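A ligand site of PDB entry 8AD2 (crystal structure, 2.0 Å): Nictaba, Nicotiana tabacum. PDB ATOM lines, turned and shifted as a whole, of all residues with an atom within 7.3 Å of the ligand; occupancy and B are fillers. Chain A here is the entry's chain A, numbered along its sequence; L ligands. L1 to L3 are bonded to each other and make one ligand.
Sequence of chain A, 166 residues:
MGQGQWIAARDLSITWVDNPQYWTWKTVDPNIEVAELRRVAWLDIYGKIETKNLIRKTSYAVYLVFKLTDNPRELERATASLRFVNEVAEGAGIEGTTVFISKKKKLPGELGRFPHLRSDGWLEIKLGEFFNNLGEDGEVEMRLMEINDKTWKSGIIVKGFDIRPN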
ATOM      1  N   THR A  15      12.897  10.283   2.833  1.00  0.00           N
ATOM      2  CA  THR A  15      12.502   9.271   1.874  1.00  0.00           C
ATOM      3  C   THR A  15      13.740   8.852   1.092  1.00  0.00           C
ATOM      4  O   THR A  15      14.641   9.661   0.837  1.00  0.00           O
ATOM      5  CB  THR A  15      11.379   9.816   0.978  1.00  0.00           C
ATOM      6  OG1 THR A  15      10.962   8.768   0.090  1.00  0.00           O
ATOM      7  CG2 THR A  15      11.849  11.000   0.169  1.00  0.00           C
ATOM      8  N   TRP A  16      13.835   7.559   0.787  1.00  0.00           N
ATOM      9  CA  TRP A  16      14.955   6.913   0.085  1.00  0.00           C
ATOM     10  C   TRP A  16      16.250   6.879   0.903  1.00  0.00           C
ATOM     11  O   TRP A  16      17.296   6.460   0.386  1.00  0.00           O
ATOM     12  CB  TRP A  16      15.250   7.608  -1.234  1.00  0.00           C
ATOM     13  CG  TRP A  16      14.098   7.569  -2.198  1.00  0.00           C
ATOM     14  CD1 TRP A  16      13.250   8.606  -2.505  1.00  0.00           C
ATOM     15  CD2 TRP A  16      13.635   6.448  -2.943  1.00  0.00           C
ATOM     16  NE1 TRP A  16      12.296   8.186  -3.416  1.00  0.00           N
ATOM     17  CE2 TRP A  16      12.526   6.876  -3.707  1.00  0.00           C
ATOM     18  CE3 TRP A  16      14.067   5.117  -3.066  1.00  0.00           C
ATOM     19  CZ2 TRP A  16      11.845   6.033  -4.542  1.00  0.00           C
ATOM     20  CZ3 TRP A  16      13.386   4.290  -3.938  1.00  0.00           C
ATOM     21  CH2 TRP A  16      12.294   4.743  -4.645  1.00  0.00           C
ATOM     22  N   ASN A  19      18.302   3.536   1.058  1.00  0.00           N
ATOM     23  CA  ASN A  19      18.722   2.899  -0.163  1.00  0.00           C
ATOM     24  C   ASN A  19      20.071   3.477  -0.526  1.00  0.00           C
ATOM     25  O   ASN A  19      20.138   4.687  -0.836  1.00  0.00           O
ATOM     26  CB  ASN A  19      17.689   3.140  -1.248  1.00  0.00           C
ATOM     27  CG  ASN A  19      18.070   2.518  -2.540  1.00  0.00           C
ATOM     28  OD1 ASN A  19      19.247   2.465  -2.893  1.00  0.00           O
ATOM     29  ND2 ASN A  19      17.070   2.074  -3.286  1.00  0.00           N
ATOM     30  N   GLN A  21      21.903   3.551  -3.065  1.00  0.00           N
ATOM     31  CA  GLN A  21      22.111   4.201  -4.361  1.00  0.00           C
ATOM     32  C   GLN A  21      21.860   5.701  -4.279  1.00  0.00           C
ATOM     33  O   GLN A  21      22.383   6.460  -5.112  1.00  0.00           O
ATOM     34  CB  GLN A  21      21.200   3.641  -5.439  1.00  0.00           C
ATOM     35  CG  GLN A  21      21.556   4.146  -6.837  1.00  0.00           C
ATOM     36  CD  GLN A  21      20.681   3.540  -7.925  1.00  0.00           C
ATOM     37  OE1 GLN A  21      19.775   4.203  -8.466  1.00  0.00           O
ATOM     38  NE2 GLN A  21      20.941   2.275  -8.261  1.00  0.00           N
ATOM     39  N   TYR A  22      21.107   6.156  -3.279  1.00  0.00           N
ATOM     40  CA  TYR A  22      20.641   7.537  -3.277  1.00  0.00           C
ATOM     41  C   TYR A  22      21.187   8.369  -2.125  1.00  0.00           C
ATOM     42  O   TYR A  22      21.442   9.569  -2.307  1.00  0.00           O
ATOM     43  CB  TYR A  22      19.095   7.567  -3.245  1.00  0.00           C
ATOM     44  CG  TYR A  22      18.435   6.922  -4.440  1.00  0.00           C
ATOM     45  CD1 TYR A  22      18.706   7.381  -5.739  1.00  0.00           C
ATOM     46  CD2 TYR A  22      17.558   5.855  -4.287  1.00  0.00           C
ATOM     47  CE1 TYR A  22      18.087   6.778  -6.836  1.00  0.00           C
ATOM     48  CE2 TYR A  22      16.939   5.248  -5.375  1.00  0.00           C
ATOM     49  CZ  TYR A  22      17.220   5.727  -6.652  1.00  0.00           C
ATOM     50  OH  TYR A  22      16.638   5.169  -7.751  1.00  0.00           O
ATOM     51  N   ARG A  39      22.161  11.214  -4.822  1.00  0.00           N
ATOM     52  CA  ARG A  39      21.213  11.732  -5.841  1.00  0.00           C
ATOM     53  C   ARG A  39      19.789  11.336  -5.469  1.00  0.00           C
ATOM     54  O   ARG A  39      19.621  10.240  -4.962  1.00  0.00           O
ATOM     55  CB  ARG A  39      21.568  11.204  -7.232  1.00  0.00           C
ATOM     56  CG  ARG A  39      21.762   9.694  -7.319  1.00  0.00           C
ATOM     57  CD  ARG A  39      22.389   9.308  -8.652  1.00  0.00           C
ATOM     58  NE  ARG A  39      21.430   9.067  -9.711  1.00  0.00           N
ATOM     59  CZ  ARG A  39      20.946   7.865 -10.019  1.00  0.00           C
ATOM     60  NH1 ARG A  39      21.333   6.803  -9.327  1.00  0.00           N
ATOM     61  NH2 ARG A  39      20.087   7.726 -11.007  1.00  0.00           N
ATOM     62  N   VAL A  40      18.819  12.224  -5.681  1.00  0.00           N
ATOM     63  CA  VAL A  40      17.388  11.880  -5.462  1.00  0.00           C
ATOM     64  C   VAL A  40      16.541  12.874  -6.277  1.00  0.00           C
ATOM     65  O   VAL A  40      16.971  14.011  -6.432  1.00  0.00           O
ATOM     66  CB  VAL A  40      16.981  11.807  -3.981  1.00  0.00           C
ATOM     67  CG1 VAL A  40      16.700  13.166  -3.379  1.00  0.00           C
ATOM     68  CG2 VAL A  40      15.818  10.867  -3.745  1.00  0.00           C
ATOM     69  N   ALA A  41      15.390  12.440  -6.786  1.00  0.00           N
ATOM     70  CA  ALA A  41      14.486  13.333  -7.538  1.00  0.00           C
ATOM     71  C   ALA A  41      13.386  13.831  -6.595  1.00  0.00           C
ATOM     72  O   ALA A  41      12.814  14.884  -6.883  1.00  0.00           O
ATOM     73  CB  ALA A  41      13.896  12.595  -8.700  1.00  0.00           C
ATOM     74  N   TRP A  42      13.139  13.081  -5.525  1.00  0.00           N
ATOM     75  CA  TRP A  42      12.122  13.426  -4.533  1.00  0.00           C
ATOM     76  C   TRP A  42      12.836  13.597  -3.187  1.00  0.00           C
ATOM     77  O   TRP A  42      13.091  12.637  -2.469  1.00  0.00           O
ATOM     78  CB  TRP A  42      11.081  12.342  -4.499  1.00  0.00           C
ATOM     79  CG  TRP A  42       9.881  12.692  -3.727  1.00  0.00           C
ATOM     80  CD1 TRP A  42       9.730  12.673  -2.363  1.00  0.00           C
ATOM     81  CD2 TRP A  42       8.614  13.113  -4.262  1.00  0.00           C
ATOM     82  NE1 TRP A  42       8.439  13.053  -2.021  1.00  0.00           N
ATOM     83  CE2 TRP A  42       7.752  13.335  -3.174  1.00  0.00           C
ATOM     84  CE3 TRP A  42       8.147  13.324  -5.559  1.00  0.00           C
ATOM     85  CZ2 TRP A  42       6.430  13.734  -3.342  1.00  0.00           C
ATOM     86  CZ3 TRP A  42       6.859  13.731  -5.724  1.00  0.00           C
ATOM     87  CH2 TRP A  42       6.007  13.941  -4.619  1.00  0.00           C
ATOM     88  N   LEU A  43      13.191  14.829  -2.877  1.00  0.00           N
ATOM     89  CA  LEU A  43      13.902  15.146  -1.660  1.00  0.00           C
ATOM     90  C   LEU A  43      12.887  15.597  -0.618  1.00  0.00           C
ATOM     91  O   LEU A  43      12.189  16.612  -0.813  1.00  0.00           O
ATOM     92  CB  LEU A  43      14.953  16.231  -1.904  1.00  0.00           C
ATOM     93  CG  LEU A  43      15.608  16.722  -0.605  1.00  0.00           C
ATOM     94  CD1 LEU A  43      16.450  15.637   0.033  1.00  0.00           C
ATOM     95  CD2 LEU A  43      16.444  17.928  -0.914  1.00  0.00           C
ATOM     96  N   ASP A  44      12.789  14.835   0.470  1.00  0.00           N
ATOM     97  CA  ASP A  44      11.873  15.220   1.536  1.00  0.00           C
ATOM     98  C   ASP A  44      12.506  14.851   2.869  1.00  0.00           C
ATOM     99  O   ASP A  44      12.654  13.662   3.145  1.00  0.00           O
ATOM    100  CB  ASP A  44      10.509  14.534   1.371  1.00  0.00           C
ATOM    101  CG  ASP A  44       9.504  14.994   2.384  1.00  0.00           C
ATOM    102  OD1 ASP A  44       9.595  16.163   2.785  1.00  0.00           O
ATOM    103  OD2 ASP A  44       8.627  14.201   2.757  1.00  0.00           O
ATOM    104  N   ARG A 143       9.383  20.287   7.417  1.00  0.00           N
ATOM    105  CA  ARG A 143      10.185  19.574   6.416  1.00  0.00           C
ATOM    106  C   ARG A 143      10.935  20.512   5.480  1.00  0.00           C
ATOM    107  O   ARG A 143      10.588  21.703   5.426  1.00  0.00           O
ATOM    108  CB  ARG A 143       9.279  18.711   5.548  1.00  0.00           C
ATOM    109  CG  ARG A 143       8.455  19.490   4.542  1.00  0.00           C
ATOM    110  CD  ARG A 143       7.070  18.894   4.453  1.00  0.00           C
ATOM    111  NE  ARG A 143       7.093  17.515   4.019  1.00  0.00           N
ATOM    112  CZ  ARG A 143       6.075  16.678   4.137  1.00  0.00           C
ATOM    113  NH1 ARG A 143       4.967  17.101   4.723  1.00  0.00           N
ATOM    114  NH2 ARG A 143       6.170  15.441   3.715  1.00  0.00           N
ATOM    115  N   ILE A 147      10.581  18.426  -4.662  1.00  0.00           N
ATOM    116  CA  ILE A 147       9.917  17.284  -5.285  1.00  0.00           C
ATOM    117  C   ILE A 147       9.648  17.533  -6.762  1.00  0.00           C
ATOM    118  O   ILE A 147       8.665  17.050  -7.317  1.00  0.00           O
ATOM    119  CB  ILE A 147       8.614  16.944  -4.543  1.00  0.00           C
ATOM    120  CG1 ILE A 147       7.749  18.178  -4.379  1.00  0.00           C
ATOM    121  CG2 ILE A 147       8.927  16.333  -3.216  1.00  0.00           C
ATOM    122  CD1 ILE A 147       6.305  17.854  -4.018  1.00  0.00           C
ATOM    123  N   ASN A 148      10.518  18.283  -7.410  1.00  0.00           N
ATOM    124  CA  ASN A 148      10.480  18.409  -8.857  1.00  0.00           C
ATOM    125  C   ASN A 148      11.025  17.119  -9.491  1.00  0.00           C
ATOM    126  O   ASN A 148      12.225  16.837  -9.411  1.00  0.00           O
ATOM    127  CB  ASN A 148      11.274  19.642  -9.286  1.00  0.00           C
ATOM    128  CG  ASN A 148      11.290  19.832 -10.790  1.00  0.00           C
ATOM    129  OD1 ASN A 148      10.816  18.993 -11.545  1.00  0.00           O
ATOM    130  ND2 ASN A 148      11.858  20.935 -11.216  1.00  0.00           N
ATOM    131  N   ASP A 149      10.141  16.313 -10.077  1.00  0.00           N
ATOM    132  CA  ASP A 149      10.499  15.002 -10.700  1.00  0.00           C
ATOM    133  C   ASP A 149      11.589  15.115 -11.749  1.00  0.00           C
ATOM    134  O   ASP A 149      12.256  14.124 -11.998  1.00  0.00           O
ATOM    135  CB  ASP A 149       9.306  14.492 -11.511  1.00  0.00           C
ATOM    136  CG  ASP A 149       8.319  13.631 -10.750  1.00  0.00           C
ATOM    137  OD1 ASP A 149       7.254  13.321 -11.322  1.00  0.00           O
ATOM    138  OD2 ASP A 149       8.624  13.294  -9.592  1.00  0.00           O
ATOM    139  N   LYS A 150      11.741  16.278 -12.358  1.00  0.00           N
ATOM    140  CA  LYS A 150      12.663  16.416 -13.508  1.00  0.00           C
ATOM    141  C   LYS A 150      14.090  16.716 -13.061  1.00  0.00           C
ATOM    142  O   LYS A 150      14.936  16.854 -13.945  1.00  0.00           O
ATOM    143  CB  LYS A 150      12.098  17.483 -14.453  1.00  0.00           C
ATOM    144  CG  LYS A 150      10.762  17.125 -15.082  1.00  0.00           C
ATOM    145  CD  LYS A 150       9.615  17.973 -14.582  1.00  0.00           C
ATOM    146  CE  LYS A 150       9.704  19.414 -15.048  1.00  0.00           C
ATOM    147  NZ  LYS A 150       8.582  20.227 -14.520  1.00  0.00           N
ATOM    148  N   THR A 151      14.333  16.846 -11.758  1.00  0.00           N
ATOM    149  CA  THR A 151      15.681  17.263 -11.312  1.00  0.00           C
ATOM    150  C   THR A 151      16.291  16.267 -10.310  1.00  0.00           C
ATOM    151  O   THR A 151      15.554  15.780  -9.460  1.00  0.00           O
ATOM    152  CB  THR A 151      15.653  18.696 -10.763  1.00  0.00           C
ATOM    153  OG1 THR A 151      14.683  18.749  -9.722  1.00  0.00           O
ATOM    154  CG2 THR A 151      15.322  19.722 -11.826  1.00  0.00           C
ATOM    155  N   TRP A 152      17.575  15.965 -10.461  1.00  0.00           N
ATOM    156  CA  TRP A 152      18.279  15.135  -9.492  1.00  0.00           C
ATOM    157  C   TRP A 152      18.953  16.078  -8.509  1.00  0.00           C
ATOM    158  O   TRP A 152      19.774  16.907  -8.909  1.00  0.00           O
ATOM    159  CB  TRP A 152      19.281  14.200 -10.177  1.00  0.00           C
ATOM    160  CG  TRP A 152      18.585  12.978 -10.828  1.00  0.00           C
ATOM    161  CD1 TRP A 152      18.224  12.817 -12.134  1.00  0.00           C
ATOM    162  CD2 TRP A 152      18.176  11.782 -10.147  1.00  0.00           C
ATOM    163  NE1 TRP A 152      17.633  11.582 -12.303  1.00  0.00           N
ATOM    164  CE2 TRP A 152      17.585  10.945 -11.101  1.00  0.00           C
ATOM    165  CE3 TRP A 152      18.271  11.352  -8.834  1.00  0.00           C
ATOM    166  CZ2 TRP A 152      17.076   9.686 -10.771  1.00  0.00           C
ATOM    167  CZ3 TRP A 152      17.760  10.122  -8.513  1.00  0.00           C
ATOM    168  CH2 TRP A 152      17.173   9.298  -9.472  1.00  0.00           C
ATOM    169  N   LYS A 153      18.531  16.037  -7.256  1.00  0.00           N
ATOM    170  CA  LYS A 153      19.166  16.839  -6.219  1.00  0.00           C
ATOM    171  C   LYS A 153      20.347  16.065  -5.664  1.00  0.00           C
ATOM    172  O   LYS A 153      20.299  14.841  -5.538  1.00  0.00           O
ATOM    173  CB  LYS A 153      18.176  17.167  -5.092  1.00  0.00           C
ATOM    174  CG  LYS A 153      17.309  18.443  -5.362  1.00  0.00           C
ATOM    175  CD  LYS A 153      16.370  18.260  -6.560  1.00  0.00           C
ATOM    176  CE  LYS A 153      15.342  17.202  -6.292  1.00  0.00           C
ATOM    177  NZ  LYS A 153      14.219  17.269  -7.305  1.00  0.00           N
HETATM  178  C1  LIG L   1      13.546  10.274 -13.039  1.00  0.00           C
HETATM  179  C2  LIG L   1      12.092  10.701 -12.951  1.00  0.00           C
HETATM  180  C3  LIG L   1      11.698  10.934 -11.502  1.00  0.00           C
HETATM  181  C4  LIG L   1      12.074   9.752 -10.624  1.00  0.00           C
HETATM  182  C5  LIG L   1      13.512   9.294 -10.881  1.00  0.00           C
HETATM  183  C6  LIG L   1      13.851   7.982 -10.220  1.00  0.00           C
HETATM  184  C7  LIG L   1      10.730  12.146 -14.406  1.00  0.00           C
HETATM  185  C8  LIG L   1      10.689  13.442 -15.173  1.00  0.00           C
HETATM  186  N1  LIG L   1      11.863  11.899 -13.744  1.00  0.00           N
HETATM  187  O1  LIG L   1      13.869  10.066 -14.378  1.00  0.00           O
HETATM  188  O2  LIG L   1      10.297  11.173 -11.415  1.00  0.00           O
HETATM  189  O3  LIG L   1      11.973  10.123  -9.251  1.00  0.00           O
HETATM  190  O4  LIG L   1      13.734   9.102 -12.289  1.00  0.00           O
HETATM  191  O5  LIG L   1      12.942   6.952 -10.613  1.00  0.00           O
HETATM  192  O6  LIG L   1       9.783  11.375 -14.388  1.00  0.00           O
HETATM  193  C1  LG2 L   2      10.835   9.505  -8.619  1.00  0.00           C
HETATM  194  C2  LG2 L   2      11.161   9.417  -7.131  1.00  0.00           C
HETATM  195  C3  LG2 L   2       9.971   8.861  -6.359  1.00  0.00           C
HETATM  196  C4  LG2 L   2       8.698   9.634  -6.682  1.00  0.00           C
HETATM  197  C5  LG2 L   2       8.504   9.714  -8.195  1.00  0.00           C
HETATM  198  C6  LG2 L   2       7.335  10.576  -8.597  1.00  0.00           C
HETATM  199  C7  LG2 L   2      13.501   9.082  -6.430  1.00  0.00           C
HETATM  200  C8  LG2 L   2      14.607   8.089  -6.268  1.00  0.00           C
HETATM  201  N1  LG2 L   2      12.348   8.598  -6.908  1.00  0.00           N
HETATM  202  O1  LG2 L   2      10.245   8.942  -4.957  1.00  0.00           O
HETATM  203  O2  LG2 L   2       7.574   8.990  -6.106  1.00  0.00           O
HETATM  204  O3  LG2 L   2       9.669  10.277  -8.809  1.00  0.00           O
HETATM  205  O4  LG2 L   2       7.319  10.781 -10.006  1.00  0.00           O
HETATM  206  O5  LG2 L   2      13.632  10.260  -6.135  1.00  0.00           O
HETATM  207  C1  LG3 L   3       7.159   9.689  -4.922  1.00  0.00           C
HETATM  208  C2  LG3 L   3       5.634   9.543  -4.786  1.00  0.00           C
HETATM  209  C3  LG3 L   3       5.143  10.105  -3.446  1.00  0.00           C
HETATM  210  C4  LG3 L   3       5.966   9.561  -2.285  1.00  0.00           C
HETATM  211  C5  LG3 L   3       7.449   9.800  -2.553  1.00  0.00           C
HETATM  212  C6  LG3 L   3       8.356   9.261  -1.478  1.00  0.00           C
HETATM  213  C7  LG3 L   3       3.975   9.669  -6.592  1.00  0.00           C
HETATM  214  C8  LG3 L   3       3.400  10.526  -7.682  1.00  0.00           C
HETATM  215  N1  LG3 L   3       4.972  10.216  -5.886  1.00  0.00           N
HETATM  216  O1  LG3 L   3       3.780   9.736  -3.283  1.00  0.00           O
HETATM  217  O2  LG3 L   3       5.594  10.223  -1.085  1.00  0.00           O
HETATM  218  O3  LG3 L   3       7.798   9.149  -3.781  1.00  0.00           O
HETATM  219  O4  LG3 L   3       8.215   7.847  -1.321  1.00  0.00           O
HETATM  220  O5  LG3 L   3       3.549   8.543  -6.366  1.00  0.00           O
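Merely in contact with the ligand: Val 40, Tyr 22, Trp 152 and Lys 150. Hydrophobic or aromatic side chains within 4 Å of the ligand: Trp 16, Tyr 22, Val 40, Ala 41, Trp 42 and Trp 152. Nine residues have an atom within 4 Å of the ligand: Thr 15, Trp 16, Tyr 22, Val 40, Ala 41, Trp 42, Asp 149, Lys 150 and Trp 152.
The backbone NH of Thr 15 lies within hydrogen-bond range of the backbone carbonyl oxygen of Asp 44, 3.4 Å away. The backbone NH (N) of Lys 153 lies within hydrogen-bond range of the backbone carbonyl oxygen (O) of Val 40, at 2.7 Å. NZ of Lys 153 is in hydrogen-bond range of O of Ala 41, at 2.8 Å. N of Arg 39 lies within hydrogen-bond range of O of Tyr 22 (3.1 Å). The side-chain amide oxygen (OD1) of Asn 148 sits at hydrogen-bond distance from the backbone NH (N) of Lys 150, 3.0 Å away. The side-chain hydroxyl (OH) of Tyr 22 lies within hydrogen-bond range of the side-chain amide oxygen (OE1) of Gln 21, at 3.4 Å.
An oxygen (O5) of LG2 L2 is in hydrogen-bond range of the backbone NH (N) of Ala 41 (2.9 Å). The backbone carbonyl oxygen of Asp 149 lies within hydrogen-bond range of a nitrogen (N1) of LIG L1 (2.9 Å). An oxygen (O1) of LG2 L2 sits at hydrogen-bond distance from the indole nitrogen (NE1) of Trp 16. The side-chain carboxylate (OD1) of Asp 149 sits at hydrogen-bond distance from an oxygen (O4) of LG2 L2, at 2.9 Å. The side-chain hydroxyl (OG1) of Thr 15 sits close to an oxygen (O4) of LG3 L3, 3.2 Å away. N of Trp 42 is in hydrogen-bond range of O5 of LG2 L2 (2.9 Å).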
